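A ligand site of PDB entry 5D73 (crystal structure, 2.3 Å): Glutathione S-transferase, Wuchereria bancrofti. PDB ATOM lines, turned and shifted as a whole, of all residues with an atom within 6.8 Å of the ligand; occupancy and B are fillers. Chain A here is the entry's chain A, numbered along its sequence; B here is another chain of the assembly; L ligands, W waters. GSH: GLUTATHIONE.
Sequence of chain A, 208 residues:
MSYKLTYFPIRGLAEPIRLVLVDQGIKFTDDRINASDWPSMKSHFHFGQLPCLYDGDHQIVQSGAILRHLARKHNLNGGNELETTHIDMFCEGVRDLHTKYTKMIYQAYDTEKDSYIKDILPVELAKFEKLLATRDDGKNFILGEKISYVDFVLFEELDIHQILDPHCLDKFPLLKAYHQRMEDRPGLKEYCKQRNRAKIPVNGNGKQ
The backbone carbonyl oxygen of Gly 48 lies close to an oxygen (O31) of the ligand (3.4 Å). Phe 8 touches the ligand. Leu 13 touches the ligand. Pro 51 touches the ligand. Of the 23 residues printed, 13 come within 4 Å of the ligand.
The side-chain hydroxyl (OG) of Ser 63 lies within hydrogen-bond range of the guanidinium group (NH2) of Arg 95, 3.4 Å away. OE1 of Gln 62 lies close to OD2 of Asp 96 of chain B, 3.0 Å away. The side-chain amide oxygen of Gln 62 sits close to the backbone carbonyl oxygen of Glu 92 of chain B (3.5 Å). NH1 of Arg 95 lies within salt-bridge range of OE2 of Glu 92 of chain B (3.5 Å). The backbone carbonyl oxygen (O) of Gly 48 is in hydrogen-bond range of the side-chain amino group (NZ) of Lys 42. The side-chain hydroxyl (OH) of Tyr 7 lies within hydrogen-bond range of the backbone NH (N) of Leu 13, 3.2 Å away.
Water W2 lies within hydrogen-bond range of the backbone carbonyl oxygen of Pro 51 (2.8 Å), an oxygen (O11) of the ligand (2.8 Å) and the backbone NH of Gln 62 (2.8 Å). Water W1 bridges the side-chain amino group of Lys 42 and an oxygen (O31) of the ligand.
The backbone NH (N) of Ser 63 sits at hydrogen-bond distance from an oxygen (O11) of the ligand. O12 of the ligand sits at hydrogen-bond distance from OG of Ser 63 (2.6 Å). N1 of the ligand lies within salt-bridge range of OD2 of Asp 96 of chain B. A nitrogen (N1) of the ligand sits close to the side-chain amide nitrogen (NE2) of Gln 62 (2.8 Å). The backbone NH (N) of Leu 50 lies within hydrogen-bond range of an oxygen (O2) of the ligand (2.9 Å). The backbone carbonyl oxygen (O) of Leu 50 lies within hydrogen-bond range of a nitrogen (N2) of the ligand (3.0 Å). An oxygen (O31) of the ligand lies close to the side-chain amide oxygen (OE1) of Gln 49, at 3.0 Å. The indole nitrogen (NE1) of Trp 38 lies within hydrogen-bond range of an oxygen (O32) of the ligand (3.1 Å). NH2 of Arg 95 is in salt-bridge range of O12 of the ligand. The side-chain amino group (NZ) of Lys 42 lies within salt-bridge range of an oxygen (O32) of the ligand, 3.3 Å away. The side-chain hydroxyl of Tyr 7 lies close to a sulfur (SG2) of the ligand (3.6 Å).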
ATOM      1  N   TYR A   7     -12.853 -12.092  25.303  1.00  0.00           N
ATOM      2  CA  TYR A   7     -13.516 -13.356  25.518  1.00  0.00           C
ATOM      3  C   TYR A   7     -12.482 -14.510  25.515  1.00  0.00           C
ATOM      4  O   TYR A   7     -11.302 -14.304  25.276  1.00  0.00           O
ATOM      5  CB  TYR A   7     -14.607 -13.557  24.447  1.00  0.00           C
ATOM      6  CG  TYR A   7     -15.619 -14.666  24.741  1.00  0.00           C
ATOM      7  CD1 TYR A   7     -16.520 -14.567  25.813  1.00  0.00           C
ATOM      8  CD2 TYR A   7     -15.671 -15.810  23.949  1.00  0.00           C
ATOM      9  CE1 TYR A   7     -17.428 -15.601  26.092  1.00  0.00           C
ATOM     10  CE2 TYR A   7     -16.586 -16.833  24.222  1.00  0.00           C
ATOM     11  CZ  TYR A   7     -17.460 -16.721  25.286  1.00  0.00           C
ATOM     12  OH  TYR A   7     -18.351 -17.714  25.535  1.00  0.00           O
ATOM     13  N   PHE A   8     -12.945 -15.715  25.828  1.00  0.00           N
ATOM     14  CA  PHE A   8     -12.162 -16.940  25.714  1.00  0.00           C
ATOM     15  C   PHE A   8     -11.867 -17.311  24.268  1.00  0.00           C
ATOM     16  O   PHE A   8     -12.560 -16.874  23.335  1.00  0.00           O
ATOM     17  CB  PHE A   8     -12.909 -18.078  26.444  1.00  0.00           C
ATOM     18  CG  PHE A   8     -13.220 -17.746  27.887  1.00  0.00           C
ATOM     19  CD1 PHE A   8     -12.193 -17.665  28.846  1.00  0.00           C
ATOM     20  CD2 PHE A   8     -14.538 -17.466  28.301  1.00  0.00           C
ATOM     21  CE1 PHE A   8     -12.481 -17.340  30.167  1.00  0.00           C
ATOM     22  CE2 PHE A   8     -14.822 -17.144  29.612  1.00  0.00           C
ATOM     23  CZ  PHE A   8     -13.799 -17.067  30.550  1.00  0.00           C
ATOM     24  N   ILE A  10     -12.677 -19.273  22.082  1.00  0.00           N
ATOM     25  CA  ILE A  10     -13.676 -20.152  21.484  1.00  0.00           C
ATOM     26  C   ILE A  10     -14.743 -19.238  20.864  1.00  0.00           C
ATOM     27  O   ILE A  10     -14.735 -18.017  21.053  1.00  0.00           O
ATOM     28  CB  ILE A  10     -14.314 -21.150  22.531  1.00  0.00           C
ATOM     29  CG1 ILE A  10     -15.262 -20.407  23.488  1.00  0.00           C
ATOM     30  CG2 ILE A  10     -13.239 -21.896  23.350  1.00  0.00           C
ATOM     31  CD1 ILE A  10     -16.017 -21.319  24.424  1.00  0.00           C
ATOM     32  N   GLY A  12     -18.389 -19.621  21.156  1.00  0.00           N
ATOM     33  CA  GLY A  12     -19.332 -19.411  22.243  1.00  0.00           C
ATOM     34  C   GLY A  12     -20.247 -18.231  22.054  1.00  0.00           C
ATOM     35  O   GLY A  12     -20.827 -18.085  20.981  1.00  0.00           O
ATOM     36  N   LEU A  13     -20.305 -17.372  23.076  1.00  0.00           N
ATOM     37  CA  LEU A  13     -21.192 -16.213  23.124  1.00  0.00           C
ATOM     38  C   LEU A  13     -20.682 -14.977  22.407  1.00  0.00           C
ATOM     39  O   LEU A  13     -21.473 -14.098  22.130  1.00  0.00           O
ATOM     40  CB  LEU A  13     -21.497 -15.815  24.580  1.00  0.00           C
ATOM     41  CG  LEU A  13     -22.257 -16.771  25.508  1.00  0.00           C
ATOM     42  CD1 LEU A  13     -22.298 -16.187  26.917  1.00  0.00           C
ATOM     43  CD2 LEU A  13     -23.671 -16.994  25.005  1.00  0.00           C
ATOM     44  N   TRP A  38      -7.351 -15.725  33.353  1.00  0.00           N
ATOM     45  CA  TRP A  38      -8.738 -15.382  33.691  1.00  0.00           C
ATOM     46  C   TRP A  38      -8.971 -15.031  35.163  1.00  0.00           C
ATOM     47  O   TRP A  38      -9.561 -13.961  35.447  1.00  0.00           O
ATOM     48  CB  TRP A  38      -9.708 -16.468  33.184  1.00  0.00           C
ATOM     49  CG  TRP A  38     -11.130 -16.251  33.620  1.00  0.00           C
ATOM     50  CD1 TRP A  38     -11.900 -17.148  34.314  1.00  0.00           C
ATOM     51  CD2 TRP A  38     -11.926 -15.074  33.459  1.00  0.00           C
ATOM     52  NE1 TRP A  38     -13.122 -16.599  34.588  1.00  0.00           N
ATOM     53  CE2 TRP A  38     -13.172 -15.321  34.088  1.00  0.00           C
ATOM     54  CE3 TRP A  38     -11.706 -13.816  32.863  1.00  0.00           C
ATOM     55  CZ2 TRP A  38     -14.203 -14.376  34.109  1.00  0.00           C
ATOM     56  CZ3 TRP A  38     -12.749 -12.867  32.890  1.00  0.00           C
ATOM     57  CH2 TRP A  38     -13.980 -13.173  33.511  1.00  0.00           C
ATOM     58  N   LYS A  42     -10.904 -11.609  36.540  1.00  0.00           N
ATOM     59  CA  LYS A  42     -12.329 -11.883  36.769  1.00  0.00           C
ATOM     60  C   LYS A  42     -13.078 -10.754  37.446  1.00  0.00           C
ATOM     61  O   LYS A  42     -14.224 -10.454  37.090  1.00  0.00           O
ATOM     62  CB  LYS A  42     -12.512 -13.182  37.567  1.00  0.00           C
ATOM     63  CG  LYS A  42     -13.973 -13.590  37.776  1.00  0.00           C
ATOM     64  CD  LYS A  42     -14.100 -14.978  38.413  1.00  0.00           C
ATOM     65  CE  LYS A  42     -15.507 -15.235  39.006  1.00  0.00           C
ATOM     66  NZ  LYS A  42     -16.687 -15.091  38.064  1.00  0.00           N
ATOM     67  N   PHE A  47     -20.155  -8.334  36.171  1.00  0.00           N
ATOM     68  CA  PHE A  47     -20.697  -9.600  36.701  1.00  0.00           C
ATOM     69  C   PHE A  47     -19.667 -10.726  36.720  1.00  0.00           C
ATOM     70  O   PHE A  47     -20.032 -11.899  36.843  1.00  0.00           O
ATOM     71  CB  PHE A  47     -21.934  -9.999  35.906  1.00  0.00           C
ATOM     72  CG  PHE A  47     -22.924  -8.896  35.798  1.00  0.00           C
ATOM     73  CD1 PHE A  47     -23.634  -8.491  36.924  1.00  0.00           C
ATOM     74  CD2 PHE A  47     -23.134  -8.254  34.583  1.00  0.00           C
ATOM     75  CE1 PHE A  47     -24.550  -7.447  36.826  1.00  0.00           C
ATOM     76  CE2 PHE A  47     -24.072  -7.217  34.480  1.00  0.00           C
ATOM     77  CZ  PHE A  47     -24.770  -6.804  35.608  1.00  0.00           C
ATOM     78  N   GLY A  48     -18.399 -10.364  36.632  1.00  0.00           N
ATOM     79  CA  GLY A  48     -17.332 -11.341  36.644  1.00  0.00           C
ATOM     80  C   GLY A  48     -17.357 -12.355  35.517  1.00  0.00           C
ATOM     81  O   GLY A  48     -16.908 -13.474  35.681  1.00  0.00           O
ATOM     82  N   GLN A  49     -17.864 -11.953  34.357  1.00  0.00           N
ATOM     83  CA  GLN A  49     -17.945 -12.843  33.203  1.00  0.00           C
ATOM     84  C   GLN A  49     -17.621 -12.079  31.883  1.00  0.00           C
ATOM     85  O   GLN A  49     -17.641 -10.827  31.842  1.00  0.00           O
ATOM     86  CB  GLN A  49     -19.347 -13.507  33.143  1.00  0.00           C
ATOM     87  CG  GLN A  49     -19.719 -14.338  34.360  1.00  0.00           C
ATOM     88  CD  GLN A  49     -20.747 -15.427  34.068  1.00  0.00           C
ATOM     89  OE1 GLN A  49     -20.488 -16.609  34.248  1.00  0.00           O
ATOM     90  NE2 GLN A  49     -21.918 -15.036  33.585  1.00  0.00           N
ATOM     91  N   LEU A  50     -17.357 -12.860  30.833  1.00  0.00           N
ATOM     92  CA  LEU A  50     -17.062 -12.391  29.462  1.00  0.00           C
ATOM     93  C   LEU A  50     -18.201 -12.912  28.585  1.00  0.00           C
ATOM     94  O   LEU A  50     -18.751 -13.939  28.920  1.00  0.00           O
ATOM     95  CB  LEU A  50     -15.695 -12.954  28.996  1.00  0.00           C
ATOM     96  CG  LEU A  50     -14.477 -12.519  29.827  1.00  0.00           C
ATOM     97  CD1 LEU A  50     -13.196 -13.048  29.201  1.00  0.00           C
ATOM     98  CD2 LEU A  50     -14.401 -10.990  29.998  1.00  0.00           C
ATOM     99  N   PRO A  51     -18.541 -12.266  27.460  1.00  0.00           N
ATOM    100  CA  PRO A  51     -17.752 -11.236  26.803  1.00  0.00           C
ATOM    101  C   PRO A  51     -17.858  -9.840  27.348  1.00  0.00           C
ATOM    102  O   PRO A  51     -18.869  -9.478  27.930  1.00  0.00           O
ATOM    103  CB  PRO A  51     -18.305 -11.237  25.359  1.00  0.00           C
ATOM    104  CG  PRO A  51     -19.693 -11.733  25.510  1.00  0.00           C
ATOM    105  CD  PRO A  51     -19.566 -12.814  26.552  1.00  0.00           C
ATOM    106  N   VAL A  61     -20.439  -5.218  29.244  1.00  0.00           N
ATOM    107  CA  VAL A  61     -20.565  -6.654  29.335  1.00  0.00           C
ATOM    108  C   VAL A  61     -22.005  -6.997  28.997  1.00  0.00           C
ATOM    109  O   VAL A  61     -22.815  -6.070  28.764  1.00  0.00           O
ATOM    110  CB  VAL A  61     -20.145  -7.210  30.719  1.00  0.00           C
ATOM    111  CG1 VAL A  61     -18.666  -6.932  30.926  1.00  0.00           C
ATOM    112  CG2 VAL A  61     -21.019  -6.663  31.855  1.00  0.00           C
ATOM    113  N   GLN A  62     -22.250  -8.311  28.909  1.00  0.00           N
ATOM    114  CA  GLN A  62     -23.525  -8.909  28.535  1.00  0.00           C
ATOM    115  C   GLN A  62     -23.684  -8.902  27.025  1.00  0.00           C
ATOM    116  O   GLN A  62     -23.841  -7.855  26.393  1.00  0.00           O
ATOM    117  CB  GLN A  62     -24.756  -8.286  29.244  1.00  0.00           C
ATOM    118  CG  GLN A  62     -24.782  -8.552  30.763  1.00  0.00           C
ATOM    119  CD  GLN A  62     -25.219  -9.969  31.147  1.00  0.00           C
ATOM    120  OE1 GLN A  62     -25.267 -10.301  32.350  1.00  0.00           O
ATOM    121  NE2 GLN A  62     -25.564 -10.791  30.151  1.00  0.00           N
ATOM    122  N   SER A  63     -23.596 -10.090  26.446  1.00  0.00           N
ATOM    123  CA  SER A  63     -23.586 -10.279  25.002  1.00  0.00           C
ATOM    124  C   SER A  63     -24.755  -9.613  24.314  1.00  0.00           C
ATOM    125  O   SER A  63     -24.594  -9.019  23.244  1.00  0.00           O
ATOM    126  CB  SER A  63     -23.558 -11.787  24.648  1.00  0.00           C
ATOM    127  OG  SER A  63     -24.640 -12.494  25.189  1.00  0.00           O
ATOM    128  N   GLY A  64     -25.948  -9.706  24.929  1.00  0.00           N
ATOM    129  CA  GLY A  64     -27.124  -9.059  24.367  1.00  0.00           C
ATOM    130  C   GLY A  64     -27.051  -7.551  24.334  1.00  0.00           C
ATOM    131  O   GLY A  64     -27.449  -6.910  23.336  1.00  0.00           O
ATOM    132  N   ILE A  66     -24.295  -5.782  24.254  1.00  0.00           N
ATOM    133  CA  ILE A  66     -23.252  -5.486  23.290  1.00  0.00           C
ATOM    134  C   ILE A  66     -23.854  -5.495  21.888  1.00  0.00           C
ATOM    135  O   ILE A  66     -23.652  -4.568  21.113  1.00  0.00           O
ATOM    136  CB  ILE A  66     -22.094  -6.519  23.383  1.00  0.00           C
ATOM    137  CG1 ILE A  66     -21.348  -6.412  24.731  1.00  0.00           C
ATOM    138  CG2 ILE A  66     -21.093  -6.317  22.261  1.00  0.00           C
ATOM    139  CD1 ILE A  66     -20.546  -7.629  25.150  1.00  0.00           C
ATOM    140  N   ARG A  95     -31.406 -17.320  21.146  1.00  0.00           N
ATOM    141  CA  ARG A  95     -30.691 -17.498  22.394  1.00  0.00           C
ATOM    142  C   ARG A  95     -31.279 -18.600  23.261  1.00  0.00           C
ATOM    143  O   ARG A  95     -30.581 -19.247  24.003  1.00  0.00           O
ATOM    144  CB  ARG A  95     -30.668 -16.179  23.139  1.00  0.00           C
ATOM    145  CG  ARG A  95     -29.952 -15.053  22.370  1.00  0.00           C
ATOM    146  CD  ARG A  95     -29.755 -13.802  23.227  1.00  0.00           C
ATOM    147  NE  ARG A  95     -28.961 -14.142  24.423  1.00  0.00           N
ATOM    148  CZ  ARG A  95     -28.284 -13.287  25.182  1.00  0.00           C
ATOM    149  NH1 ARG A  95     -28.259 -11.997  24.922  1.00  0.00           N
ATOM    150  NH2 ARG A  95     -27.606 -13.753  26.230  1.00  0.00           N
ATOM    151  N   TYR A 106     -22.477 -29.353  27.468  1.00  0.00           N
ATOM    152  CA  TYR A 106     -21.724 -29.375  28.741  1.00  0.00           C
ATOM    153  C   TYR A 106     -22.143 -30.500  29.725  1.00  0.00           C
ATOM    154  O   TYR A 106     -21.322 -31.023  30.452  1.00  0.00           O
ATOM    155  CB  TYR A 106     -21.772 -27.995  29.442  1.00  0.00           C
ATOM    156  CG  TYR A 106     -20.958 -26.917  28.710  1.00  0.00           C
ATOM    157  CD1 TYR A 106     -19.552 -26.872  28.808  1.00  0.00           C
ATOM    158  CD2 TYR A 106     -21.581 -25.978  27.891  1.00  0.00           C
ATOM    159  CE1 TYR A 106     -18.812 -25.904  28.112  1.00  0.00           C
ATOM    160  CE2 TYR A 106     -20.855 -25.027  27.197  1.00  0.00           C
ATOM    161  CZ  TYR A 106     -19.471 -24.977  27.297  1.00  0.00           C
ATOM    162  OH  TYR A 106     -18.768 -23.990  26.594  1.00  0.00           O
ATOM    163  N   GLU B  92     -29.958  -7.533  31.920  1.00  0.00           N
ATOM    164  CA  GLU B  92     -29.404  -8.849  31.600  1.00  0.00           C
ATOM    165  C   GLU B  92     -28.702  -9.495  32.796  1.00  0.00           C
ATOM    166  O   GLU B  92     -28.688 -10.713  32.922  1.00  0.00           O
ATOM    167  CB  GLU B  92     -28.451  -8.757  30.413  1.00  0.00           C
ATOM    168  CG  GLU B  92     -29.119  -8.562  29.074  1.00  0.00           C
ATOM    169  CD  GLU B  92     -29.966  -9.761  28.623  1.00  0.00           C
ATOM    170  OE1 GLU B  92     -31.112  -9.864  29.047  1.00  0.00           O
ATOM    171  OE2 GLU B  92     -29.538 -10.615  27.827  1.00  0.00           O
ATOM    172  N   GLY B  93     -28.132  -8.676  33.677  1.00  0.00           N
ATOM    173  CA  GLY B  93     -27.575  -9.164  34.926  1.00  0.00           C
ATOM    174  C   GLY B  93     -28.659  -9.744  35.788  1.00  0.00           C
ATOM    175  O   GLY B  93     -28.542 -10.836  36.334  1.00  0.00           O
ATOM    176  N   ASP B  96     -29.862 -13.117  34.538  1.00  0.00           N
ATOM    177  CA  ASP B  96     -28.924 -14.195  34.854  1.00  0.00           C
ATOM    178  C   ASP B  96     -29.125 -14.756  36.253  1.00  0.00           C
ATOM    179  O   ASP B  96     -29.048 -15.974  36.443  1.00  0.00           O
ATOM    180  CB  ASP B  96     -27.459 -13.795  34.660  1.00  0.00           C
ATOM    181  CG  ASP B  96     -27.047 -13.726  33.177  1.00  0.00           C
ATOM    182  OD1 ASP B  96     -27.828 -14.201  32.343  1.00  0.00           O
ATOM    183  OD2 ASP B  96     -25.972 -13.199  32.839  1.00  0.00           O
ATOM    184  N   LYS B 127     -22.597  -7.936  43.310  1.00  0.00           N
ATOM    185  CA  LYS B 127     -22.465  -7.394  41.973  1.00  0.00           C
ATOM    186  C   LYS B 127     -23.492  -6.289  41.675  1.00  0.00           C
ATOM    187  O   LYS B 127     -23.153  -5.240  41.134  1.00  0.00           O
ATOM    188  CB  LYS B 127     -22.545  -8.505  40.950  1.00  0.00           C
ATOM    189  CG  LYS B 127     -21.330  -9.440  40.906  1.00  0.00           C
ATOM    190  CD  LYS B 127     -21.722 -10.733  40.179  1.00  0.00           C
ATOM    191  CE  LYS B 127     -20.590 -11.756  40.084  1.00  0.00           C
ATOM    192  NZ  LYS B 127     -20.900 -12.864  39.131  1.00  0.00           N
HETATM  193  N1  GSH L   1     -25.313 -13.616  30.277  1.00  0.00           N
HETATM  194  CA1 GSH L   1     -23.912 -13.484  29.934  1.00  0.00           C
HETATM  195  C1  GSH L   1     -23.791 -13.028  28.502  1.00  0.00           C
HETATM  196  O11 GSH L   1     -22.784 -12.326  28.192  1.00  0.00           O
HETATM  197  O12 GSH L   1     -24.710 -13.324  27.683  1.00  0.00           O
HETATM  198  CB1 GSH L   1     -23.264 -14.841  30.155  1.00  0.00           C
HETATM  199  CG1 GSH L   1     -21.749 -14.715  30.226  1.00  0.00           C
HETATM  200  CD1 GSH L   1     -21.136 -16.049  30.582  1.00  0.00           C
HETATM  201  OE1 GSH L   1     -21.836 -16.984  30.837  1.00  0.00           O
HETATM  202  N2  GSH L   1     -19.833 -16.119  30.588  1.00  0.00           N
HETATM  203  CA2 GSH L   1     -19.074 -17.306  30.961  1.00  0.00           C
HETATM  204  C2  GSH L   1     -17.901 -16.829  31.786  1.00  0.00           C
HETATM  205  O2  GSH L   1     -17.515 -15.690  31.593  1.00  0.00           O
HETATM  206  CB2 GSH L   1     -18.624 -18.032  29.698  1.00  0.00           C
HETATM  207  SG2 GSH L   1     -19.928 -18.769  28.645  1.00  0.00           S
HETATM  208  N3  GSH L   1     -17.346 -17.661  32.658  1.00  0.00           N
HETATM  209  CA3 GSH L   1     -16.203 -17.387  33.532  1.00  0.00           C
HETATM  210  C3  GSH L   1     -16.538 -17.201  35.007  1.00  0.00           C
HETATM  211  O31 GSH L   1     -17.629 -16.730  35.272  1.00  0.00           O
HETATM  212  O32 GSH L   1     -15.768 -17.473  35.952  1.00  0.00           O
HETATM  213  O   HOH W   1     -19.159 -16.431  37.743  1.00  0.00           O
HETATM  214  O   HOH W   2     -20.849 -10.714  29.463  1.00  0.00           O
HETATM  215  O   HOH W   3     -17.738 -19.042  38.298  1.00  0.00           O
HETATM  216  O   HOH W   4     -16.849 -20.150  27.689  1.00  0.00           O
HETATM  217  O   HOH W   5     -26.905 -10.949  27.451  1.00  0.00           O
